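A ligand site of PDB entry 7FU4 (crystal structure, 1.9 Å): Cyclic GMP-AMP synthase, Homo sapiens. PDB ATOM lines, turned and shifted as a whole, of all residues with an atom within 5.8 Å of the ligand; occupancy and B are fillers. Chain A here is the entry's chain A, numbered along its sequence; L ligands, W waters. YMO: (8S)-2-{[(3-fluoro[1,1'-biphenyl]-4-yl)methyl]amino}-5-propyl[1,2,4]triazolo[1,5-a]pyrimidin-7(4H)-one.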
ATOM      1  N   ALA A  87      20.293  -0.640  10.744  1.00  0.00           N
ATOM      2  CA  ALA A  87      19.986  -0.103   9.416  1.00  0.00           C
ATOM      3  C   ALA A  87      19.050   1.099   9.419  1.00  0.00           C
ATOM      4  O   ALA A  87      18.919   1.758   8.379  1.00  0.00           O
ATOM      5  CB  ALA A  87      19.351  -1.200   8.547  1.00  0.00           C
ATOM      6  N   TYR A  88      18.368   1.378  10.535  1.00  0.00           N
ATOM      7  CA  TYR A  88      17.379   2.437  10.631  1.00  0.00           C
ATOM      8  C   TYR A  88      17.895   3.525  11.559  1.00  0.00           C
ATOM      9  O   TYR A  88      18.489   3.232  12.617  1.00  0.00           O
ATOM     10  CB  TYR A  88      16.056   1.883  11.170  1.00  0.00           C
ATOM     11  CG  TYR A  88      15.389   0.930  10.202  1.00  0.00           C
ATOM     12  CD1 TYR A  88      15.715  -0.429  10.204  1.00  0.00           C
ATOM     13  CD2 TYR A  88      14.446   1.392   9.287  1.00  0.00           C
ATOM     14  CE1 TYR A  88      15.085  -1.311   9.304  1.00  0.00           C
ATOM     15  CE2 TYR A  88      13.819   0.534   8.381  1.00  0.00           C
ATOM     16  CZ  TYR A  88      14.141  -0.808   8.395  1.00  0.00           C
ATOM     17  OH  TYR A  88      13.522  -1.656   7.500  1.00  0.00           O
ATOM     18  N   ARG A 216      16.252   4.521   6.358  1.00  0.00           N
ATOM     19  CA  ARG A 216      17.028   3.309   6.164  1.00  0.00           C
ATOM     20  C   ARG A 216      18.173   3.574   5.192  1.00  0.00           C
ATOM     21  O   ARG A 216      17.995   4.259   4.180  1.00  0.00           O
ATOM     22  CB  ARG A 216      16.152   2.156   5.639  1.00  0.00           C
ATOM     23  CG  ARG A 216      16.893   0.822   5.562  1.00  0.00           C
ATOM     24  CD  ARG A 216      15.912  -0.316   5.362  1.00  0.00           C
ATOM     25  NE  ARG A 216      15.508  -0.483   3.960  1.00  0.00           N
ATOM     26  CZ  ARG A 216      14.460  -1.235   3.598  1.00  0.00           C
ATOM     27  NH1 ARG A 216      13.730  -1.825   4.521  1.00  0.00           N
ATOM     28  NH2 ARG A 216      14.135  -1.370   2.316  1.00  0.00           N
ATOM     29  N   LEU A 217      19.352   3.030   5.509  1.00  0.00           N
ATOM     30  CA  LEU A 217      20.511   3.178   4.631  1.00  0.00           C
ATOM     31  C   LEU A 217      20.237   2.489   3.307  1.00  0.00           C
ATOM     32  O   LEU A 217      19.616   1.419   3.250  1.00  0.00           O
ATOM     33  CB  LEU A 217      21.765   2.592   5.261  1.00  0.00           C
ATOM     34  CG  LEU A 217      22.223   3.136   6.611  1.00  0.00           C
ATOM     35  CD1 LEU A 217      23.354   2.255   7.127  1.00  0.00           C
ATOM     36  CD2 LEU A 217      22.702   4.560   6.456  1.00  0.00           C
ATOM     37  N   SER A 218      20.716   3.103   2.223  1.00  0.00           N
ATOM     38  CA  SER A 218      20.490   2.585   0.889  1.00  0.00           C
ATOM     39  C   SER A 218      21.798   2.692   0.115  1.00  0.00           C
ATOM     40  O   SER A 218      22.443   3.744   0.126  1.00  0.00           O
ATOM     41  CB  SER A 218      19.366   3.373   0.188  1.00  0.00           C
ATOM     42  OG  SER A 218      19.316   3.084  -1.188  1.00  0.00           O
ATOM     43  N   PHE A 219      22.208   1.592  -0.510  1.00  0.00           N
ATOM     44  CA  PHE A 219      23.477   1.576  -1.228  1.00  0.00           C
ATOM     45  C   PHE A 219      23.292   1.084  -2.663  1.00  0.00           C
ATOM     46  O   PHE A 219      24.113   0.324  -3.180  1.00  0.00           O
ATOM     47  CB  PHE A 219      24.502   0.697  -0.512  1.00  0.00           C
ATOM     48  CG  PHE A 219      24.884   1.177   0.856  1.00  0.00           C
ATOM     49  CD1 PHE A 219      25.814   2.192   1.032  1.00  0.00           C
ATOM     50  CD2 PHE A 219      24.330   0.578   1.987  1.00  0.00           C
ATOM     51  CE1 PHE A 219      26.175   2.619   2.302  1.00  0.00           C
ATOM     52  CE2 PHE A 219      24.682   1.002   3.267  1.00  0.00           C
ATOM     53  CZ  PHE A 219      25.611   2.019   3.424  1.00  0.00           C
ATOM     54  N   SER A 220      22.211   1.514  -3.339  1.00  0.00           N
ATOM     55  CA  SER A 220      21.916   0.945  -4.665  1.00  0.00           C
ATOM     56  C   SER A 220      22.911   1.414  -5.717  1.00  0.00           C
ATOM     57  O   SER A 220      23.077   0.748  -6.748  1.00  0.00           O
ATOM     58  CB  SER A 220      20.499   1.311  -5.101  1.00  0.00           C
ATOM     59  OG  SER A 220      20.391   2.721  -5.264  1.00  0.00           O
ATOM     60  N   HIS A 221      23.591   2.522  -5.478  1.00  0.00           N
ATOM     61  CA  HIS A 221      24.623   2.988  -6.392  1.00  0.00           C
ATOM     62  C   HIS A 221      25.878   2.124  -6.299  1.00  0.00           C
ATOM     63  O   HIS A 221      26.581   1.978  -7.306  1.00  0.00           O
ATOM     64  CB  HIS A 221      24.978   4.441  -6.088  1.00  0.00           C
ATOM     65  CG  HIS A 221      25.467   4.672  -4.694  1.00  0.00           C
ATOM     66  ND1 HIS A 221      24.809   4.193  -3.567  1.00  0.00           N
ATOM     67  CD2 HIS A 221      26.538   5.352  -4.232  1.00  0.00           C
ATOM     68  CE1 HIS A 221      25.471   4.552  -2.492  1.00  0.00           C
ATOM     69  NE2 HIS A 221      26.532   5.262  -2.866  1.00  0.00           N
ATOM     70  N   GLU A 223      25.805  -1.139  -5.507  1.00  0.00           N
ATOM     71  CA  GLU A 223      25.399  -2.338  -6.227  1.00  0.00           C
ATOM     72  C   GLU A 223      25.588  -2.179  -7.728  1.00  0.00           C
ATOM     73  O   GLU A 223      26.117  -3.072  -8.404  1.00  0.00           O
ATOM     74  CB  GLU A 223      23.932  -2.659  -5.927  1.00  0.00           C
ATOM     75  CG  GLU A 223      23.439  -3.819  -6.766  1.00  0.00           C
ATOM     76  CD  GLU A 223      21.914  -3.995  -6.735  1.00  0.00           C
ATOM     77  OE1 GLU A 223      21.400  -4.800  -7.542  1.00  0.00           O
ATOM     78  OE2 GLU A 223      21.248  -3.350  -5.912  1.00  0.00           O
ATOM     79  N   SER A 274      11.489 -10.136  -1.532  1.00  0.00           N
ATOM     80  CA  SER A 274      11.705  -9.145  -2.581  1.00  0.00           C
ATOM     81  C   SER A 274      13.070  -9.391  -3.218  1.00  0.00           C
ATOM     82  O   SER A 274      13.821 -10.299  -2.819  1.00  0.00           O
ATOM     83  CB  SER A 274      11.624  -7.731  -2.026  1.00  0.00           C
ATOM     84  OG  SER A 274      12.824  -7.432  -1.335  1.00  0.00           O
ATOM     85  N   TYR A 276      15.671  -7.699  -2.839  1.00  0.00           N
ATOM     86  CA  TYR A 276      16.750  -7.562  -1.858  1.00  0.00           C
ATOM     87  C   TYR A 276      17.247  -8.912  -1.392  1.00  0.00           C
ATOM     88  O   TYR A 276      18.441  -9.092  -1.165  1.00  0.00           O
ATOM     89  CB  TYR A 276      16.305  -6.791  -0.629  1.00  0.00           C
ATOM     90  CG  TYR A 276      16.373  -5.293  -0.732  1.00  0.00           C
ATOM     91  CD1 TYR A 276      17.586  -4.616  -0.606  1.00  0.00           C
ATOM     92  CD2 TYR A 276      15.208  -4.543  -0.879  1.00  0.00           C
ATOM     93  CE1 TYR A 276      17.632  -3.224  -0.672  1.00  0.00           C
ATOM     94  CE2 TYR A 276      15.247  -3.166  -0.926  1.00  0.00           C
ATOM     95  CZ  TYR A 276      16.455  -2.508  -0.823  1.00  0.00           C
ATOM     96  OH  TYR A 276      16.486  -1.142  -0.881  1.00  0.00           O
ATOM     97  N   HIS A 277      16.325  -9.867  -1.216  1.00  0.00           N
ATOM     98  CA  HIS A 277      16.745 -11.146  -0.662  1.00  0.00           C
ATOM     99  C   HIS A 277      17.546 -11.945  -1.680  1.00  0.00           C
ATOM    100  O   HIS A 277      18.575 -12.542  -1.339  1.00  0.00           O
ATOM    101  CB  HIS A 277      15.519 -11.919  -0.163  1.00  0.00           C
ATOM    102  CG  HIS A 277      14.754 -11.179   0.884  1.00  0.00           C
ATOM    103  ND1 HIS A 277      13.577 -10.518   0.624  1.00  0.00           N
ATOM    104  CD2 HIS A 277      15.040 -10.932   2.184  1.00  0.00           C
ATOM    105  CE1 HIS A 277      13.145  -9.931   1.724  1.00  0.00           C
ATOM    106  NE2 HIS A 277      14.018 -10.158   2.689  1.00  0.00           N
ATOM    107  N   LYS A 279      19.134 -10.642  -4.461  1.00  0.00           N
ATOM    108  CA  LYS A 279      20.385  -9.926  -4.707  1.00  0.00           C
ATOM    109  C   LYS A 279      21.412 -10.206  -3.621  1.00  0.00           C
ATOM    110  O   LYS A 279      22.577 -10.468  -3.900  1.00  0.00           O
ATOM    111  CB  LYS A 279      20.151  -8.417  -4.776  1.00  0.00           C
ATOM    112  CG  LYS A 279      19.343  -7.913  -5.928  1.00  0.00           C
ATOM    113  CD  LYS A 279      19.190  -6.406  -5.790  1.00  0.00           C
ATOM    114  CE  LYS A 279      18.366  -5.797  -6.905  1.00  0.00           C
ATOM    115  NZ  LYS A 279      18.286  -4.333  -6.779  1.00  0.00           N
ATOM    116  N   THR A 280      20.982 -10.117  -2.349  1.00  0.00           N
ATOM    117  CA  THR A 280      21.907 -10.323  -1.244  1.00  0.00           C
ATOM    118  C   THR A 280      22.526 -11.702  -1.298  1.00  0.00           C
ATOM    119  O   THR A 280      23.740 -11.852  -1.159  1.00  0.00           O
ATOM    120  CB  THR A 280      21.178 -10.151   0.073  1.00  0.00           C
ATOM    121  OG1 THR A 280      20.733  -8.797   0.171  1.00  0.00           O
ATOM    122  CG2 THR A 280      22.116 -10.476   1.231  1.00  0.00           C
ATOM    123  N   PHE A 283      25.238 -11.909  -4.018  1.00  0.00           N
ATOM    124  CA  PHE A 283      26.517 -11.262  -3.729  1.00  0.00           C
ATOM    125  C   PHE A 283      27.342 -12.051  -2.731  1.00  0.00           C
ATOM    126  O   PHE A 283      28.576 -12.074  -2.829  1.00  0.00           O
ATOM    127  CB  PHE A 283      26.302  -9.821  -3.231  1.00  0.00           C
ATOM    128  CG  PHE A 283      26.139  -8.813  -4.340  1.00  0.00           C
ATOM    129  CD1 PHE A 283      24.926  -8.663  -4.985  1.00  0.00           C
ATOM    130  CD2 PHE A 283      27.195  -8.008  -4.730  1.00  0.00           C
ATOM    131  CE1 PHE A 283      24.774  -7.766  -6.040  1.00  0.00           C
ATOM    132  CE2 PHE A 283      27.038  -7.086  -5.751  1.00  0.00           C
ATOM    133  CZ  PHE A 283      25.820  -6.958  -6.399  1.00  0.00           C
ATOM    134  N   ASN A 322      22.579  -9.030   5.629  1.00  0.00           N
ATOM    135  CA  ASN A 322      22.722  -7.901   4.707  1.00  0.00           C
ATOM    136  C   ASN A 322      24.187  -7.749   4.282  1.00  0.00           C
ATOM    137  O   ASN A 322      25.101  -7.918   5.089  1.00  0.00           O
ATOM    138  CB  ASN A 322      22.221  -6.609   5.347  1.00  0.00           C
ATOM    139  CG  ASN A 322      22.307  -5.420   4.418  1.00  0.00           C
ATOM    140  OD1 ASN A 322      23.346  -4.782   4.319  1.00  0.00           O
ATOM    141  ND2 ASN A 322      21.209  -5.126   3.714  1.00  0.00           N
ATOM    142  N   TYR A 323      24.400  -7.451   2.992  1.00  0.00           N
ATOM    143  CA  TYR A 323      25.760  -7.471   2.438  1.00  0.00           C
ATOM    144  C   TYR A 323      26.607  -6.291   2.939  1.00  0.00           C
ATOM    145  O   TYR A 323      27.840  -6.373   2.944  1.00  0.00           O
ATOM    146  CB  TYR A 323      25.679  -7.469   0.895  1.00  0.00           C
ATOM    147  CG  TYR A 323      26.956  -7.946   0.191  1.00  0.00           C
ATOM    148  CD1 TYR A 323      27.331  -9.287   0.222  1.00  0.00           C
ATOM    149  CD2 TYR A 323      27.806  -7.025  -0.461  1.00  0.00           C
ATOM    150  CE1 TYR A 323      28.496  -9.714  -0.385  1.00  0.00           C
ATOM    151  CE2 TYR A 323      28.984  -7.465  -1.101  1.00  0.00           C
ATOM    152  CZ  TYR A 323      29.315  -8.798  -1.056  1.00  0.00           C
ATOM    153  OH  TYR A 323      30.474  -9.239  -1.654  1.00  0.00           O
ATOM    154  N   PHE A 324      25.962  -5.194   3.339  1.00  0.00           N
ATOM    155  CA  PHE A 324      26.621  -4.003   3.866  1.00  0.00           C
ATOM    156  C   PHE A 324      26.612  -3.941   5.385  1.00  0.00           C
ATOM    157  O   PHE A 324      27.503  -3.342   5.991  1.00  0.00           O
ATOM    158  CB  PHE A 324      25.955  -2.728   3.331  1.00  0.00           C
ATOM    159  CG  PHE A 324      26.022  -2.618   1.811  1.00  0.00           C
ATOM    160  CD1 PHE A 324      25.048  -3.200   1.032  1.00  0.00           C
ATOM    161  CD2 PHE A 324      27.066  -1.957   1.198  1.00  0.00           C
ATOM    162  CE1 PHE A 324      25.100  -3.129  -0.340  1.00  0.00           C
ATOM    163  CE2 PHE A 324      27.127  -1.882  -0.184  1.00  0.00           C
ATOM    164  CZ  PHE A 324      26.150  -2.489  -0.946  1.00  0.00           C
ATOM    165  N   ILE A 325      25.628  -4.549   6.022  1.00  0.00           N
ATOM    166  CA  ILE A 325      25.462  -4.454   7.477  1.00  0.00           C
ATOM    167  C   ILE A 325      25.341  -5.884   7.979  1.00  0.00           C
ATOM    168  O   ILE A 325      24.224  -6.430   8.026  1.00  0.00           O
ATOM    169  CB  ILE A 325      24.234  -3.625   7.832  1.00  0.00           C
ATOM    170  CG1 ILE A 325      24.281  -2.255   7.135  1.00  0.00           C
ATOM    171  CG2 ILE A 325      24.030  -3.529   9.351  1.00  0.00           C
ATOM    172  CD1 ILE A 325      23.009  -1.441   7.320  1.00  0.00           C
ATOM    173  N   PHE A 328      22.554  -7.327  10.376  1.00  0.00           N
ATOM    174  CA  PHE A 328      21.157  -7.308   9.989  1.00  0.00           C
ATOM    175  C   PHE A 328      20.845  -8.628   9.265  1.00  0.00           C
ATOM    176  O   PHE A 328      21.353  -8.872   8.168  1.00  0.00           O
ATOM    177  CB  PHE A 328      20.858  -6.107   9.081  1.00  0.00           C
ATOM    178  CG  PHE A 328      19.413  -5.811   9.032  1.00  0.00           C
ATOM    179  CD1 PHE A 328      18.571  -6.514   8.175  1.00  0.00           C
ATOM    180  CD2 PHE A 328      18.861  -4.882   9.897  1.00  0.00           C
ATOM    181  CE1 PHE A 328      17.195  -6.279   8.162  1.00  0.00           C
ATOM    182  CE2 PHE A 328      17.500  -4.626   9.907  1.00  0.00           C
ATOM    183  CZ  PHE A 328      16.655  -5.316   9.031  1.00  0.00           C
ATOM    184  N   LEU A 330      18.305 -10.553   7.278  1.00  0.00           N
ATOM    185  CA  LEU A 330      17.121 -10.387   6.450  1.00  0.00           C
ATOM    186  C   LEU A 330      16.092 -11.473   6.687  1.00  0.00           C
ATOM    187  O   LEU A 330      14.897 -11.247   6.497  1.00  0.00           O
ATOM    188  CB  LEU A 330      17.543 -10.360   4.973  1.00  0.00           C
ATOM    189  CG  LEU A 330      18.370  -9.153   4.577  1.00  0.00           C
ATOM    190  CD1 LEU A 330      18.842  -9.310   3.150  1.00  0.00           C
ATOM    191  CD2 LEU A 330      17.513  -7.922   4.719  1.00  0.00           C
ATOM    192  N   LEU A 335      11.289 -10.703  11.047  1.00  0.00           N
ATOM    193  CA  LEU A 335      11.087 -10.089   9.733  1.00  0.00           C
ATOM    194  C   LEU A 335      10.204 -10.990   8.870  1.00  0.00           C
ATOM    195  O   LEU A 335       9.125 -10.575   8.415  1.00  0.00           O
ATOM    196  CB  LEU A 335      12.442  -9.792   9.084  1.00  0.00           C
ATOM    197  CG  LEU A 335      13.239  -8.606   9.660  1.00  0.00           C
ATOM    198  CD1 LEU A 335      14.543  -8.406   8.890  1.00  0.00           C
ATOM    199  CD2 LEU A 335      12.445  -7.315   9.664  1.00  0.00           C
HETATM  200  C10 YMO L   1      14.105  -5.824   3.358  1.00  0.00           C
HETATM  201  C11 YMO L   1      13.479  -5.976   4.580  1.00  0.00           C
HETATM  202  C13 YMO L   1      15.250  -4.765   5.642  1.00  0.00           C
HETATM  203  C16 YMO L   1      21.160  -1.673   1.571  1.00  0.00           C
HETATM  204  C19 YMO L   1      21.297  -2.146  -1.831  1.00  0.00           C
HETATM  205  C21 YMO L   1      21.544  -3.449  -2.423  1.00  0.00           C
HETATM  206  C22 YMO L   1      21.752  -4.563  -1.678  1.00  0.00           C
HETATM  207  C24 YMO L   1      21.465  -3.292   0.321  1.00  0.00           C
HETATM  208  C26 YMO L   1      22.002  -5.947  -2.221  1.00  0.00           C
HETATM  209  C27 YMO L   1      23.449  -6.412  -2.217  1.00  0.00           C
HETATM  210  C28 YMO L   1      24.384  -5.617  -3.116  1.00  0.00           C
HETATM  211  C12 YMO L   1      14.045  -5.442   5.718  1.00  0.00           C
HETATM  212  C14 YMO L   1      21.007  -1.704   4.071  1.00  0.00           C
HETATM  213  C2  YMO L   1      19.351  -3.262   5.250  1.00  0.00           C
HETATM  214  C3  YMO L   1      19.673  -2.440   4.179  1.00  0.00           C
HETATM  215  C4  YMO L   1      18.709  -2.344   3.172  1.00  0.00           C
HETATM  216  C5  YMO L   1      17.508  -3.041   3.245  1.00  0.00           C
HETATM  217  C6  YMO L   1      17.207  -3.861   4.335  1.00  0.00           C
HETATM  218  C7  YMO L   1      18.163  -3.960   5.352  1.00  0.00           C
HETATM  219  C8  YMO L   1      15.913  -4.594   4.420  1.00  0.00           C
HETATM  220  C9  YMO L   1      15.320  -5.144   3.282  1.00  0.00           C
HETATM  221  F1  YMO L   1      20.259  -3.380   6.238  1.00  0.00           F
HETATM  222  N15 YMO L   1      21.037  -0.985   2.795  1.00  0.00           N
HETATM  223  N17 YMO L   1      21.065  -1.095   0.385  1.00  0.00           N
HETATM  224  N18 YMO L   1      21.300  -2.187  -0.429  1.00  0.00           N
HETATM  225  N23 YMO L   1      21.704  -4.489  -0.295  1.00  0.00           N
HETATM  226  N25 YMO L   1      21.391  -3.019   1.602  1.00  0.00           N
HETATM  227  O20 YMO L   1      21.088  -1.080  -2.411  1.00  0.00           O
HETATM  228  O   HOH W   1      22.230  -6.859   1.217  1.00  0.00           O
HETATM  229  O   HOH W   2      19.368  -2.168  -4.777  1.00  0.00           O
HETATM  230  O   HOH W   3      18.993   0.166  -1.554  1.00  0.00           O
HETATM  231  O   HOH W   4      13.756  -9.286   5.054  1.00  0.00           O
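The backbone carbonyl oxygen (O) of Leu 217 sits at hydrogen-bond distance from a nitrogen (N15) of the ligand (2.8 Å). An oxygen (O20) of the ligand is in hydrogen-bond range of the backbone NH (N) of Ser 220 (3.0 Å). A nitrogen (N25) of the ligand sits at hydrogen-bond distance from the side-chain amide nitrogen of Asn 322, 3.0 Å away. N of Phe 219 sits at hydrogen-bond distance from N17 of the ligand (3.1 Å).
The backbone carbonyl oxygen (O) of Ala 87 lies within hydrogen-bond range of the backbone NH (N) of Leu 217 (3.2 Å). The backbone NH (N) of Asn 322 lies within hydrogen-bond range of the backbone carbonyl oxygen (O) of Phe 328 (2.8 Å). The side-chain amide oxygen of Asn 322 lies within hydrogen-bond range of the backbone NH of Ile 325, 2.9 Å away. OD1 of Asn 322 lies within hydrogen-bond range of N of Phe 324, 2.8 Å away. OH of Tyr 88 sits at hydrogen-bond distance from NH1 of Arg 216 (3.0 Å). NZ of Lys 279 is in salt-bridge range of OE2 of Glu 223 (3.2 Å). OG1 of Thr 280 sits at hydrogen-bond distance from O of Tyr 276 (2.7 Å). The backbone NH (N) of Tyr 276 lies close to the side-chain hydroxyl (OG) of Ser 274.
Merely in contact with the ligand: Ala 87, Arg 216, Glu 223, Phe 328, Ile 325, Phe 283, Phe 324, Leu 330, Ser 218, Tyr 276, Thr 280 and Tyr 323. Hydrophobic or aromatic side chains within 4 Å of the ligand: Ala 87, Phe 219, Tyr 276, Phe 283, Tyr 323, Phe 324, Ile 325, Phe 328 and Leu 330. Of the 22 residues printed, 16 come within 4 Å of the ligand. The nearest printed residue that does not touch the ligand is Lys 279 (4.01 Å).
Water W3 lies within hydrogen-bond range of O20 of the ligand (2.6 Å), OH of Tyr 276 (2.9 Å) and OG of Ser 218 (3.0 Å). Water W2 lies within hydrogen-bond range of OE2 of Glu 223 (2.5 Å), O20 of the ligand (3.1 Å) and NZ of Lys 279 (3.1 Å). Water W4 bridges NE2 of His 277 (2.5 Å) and O of Leu 330 (2.7 Å).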
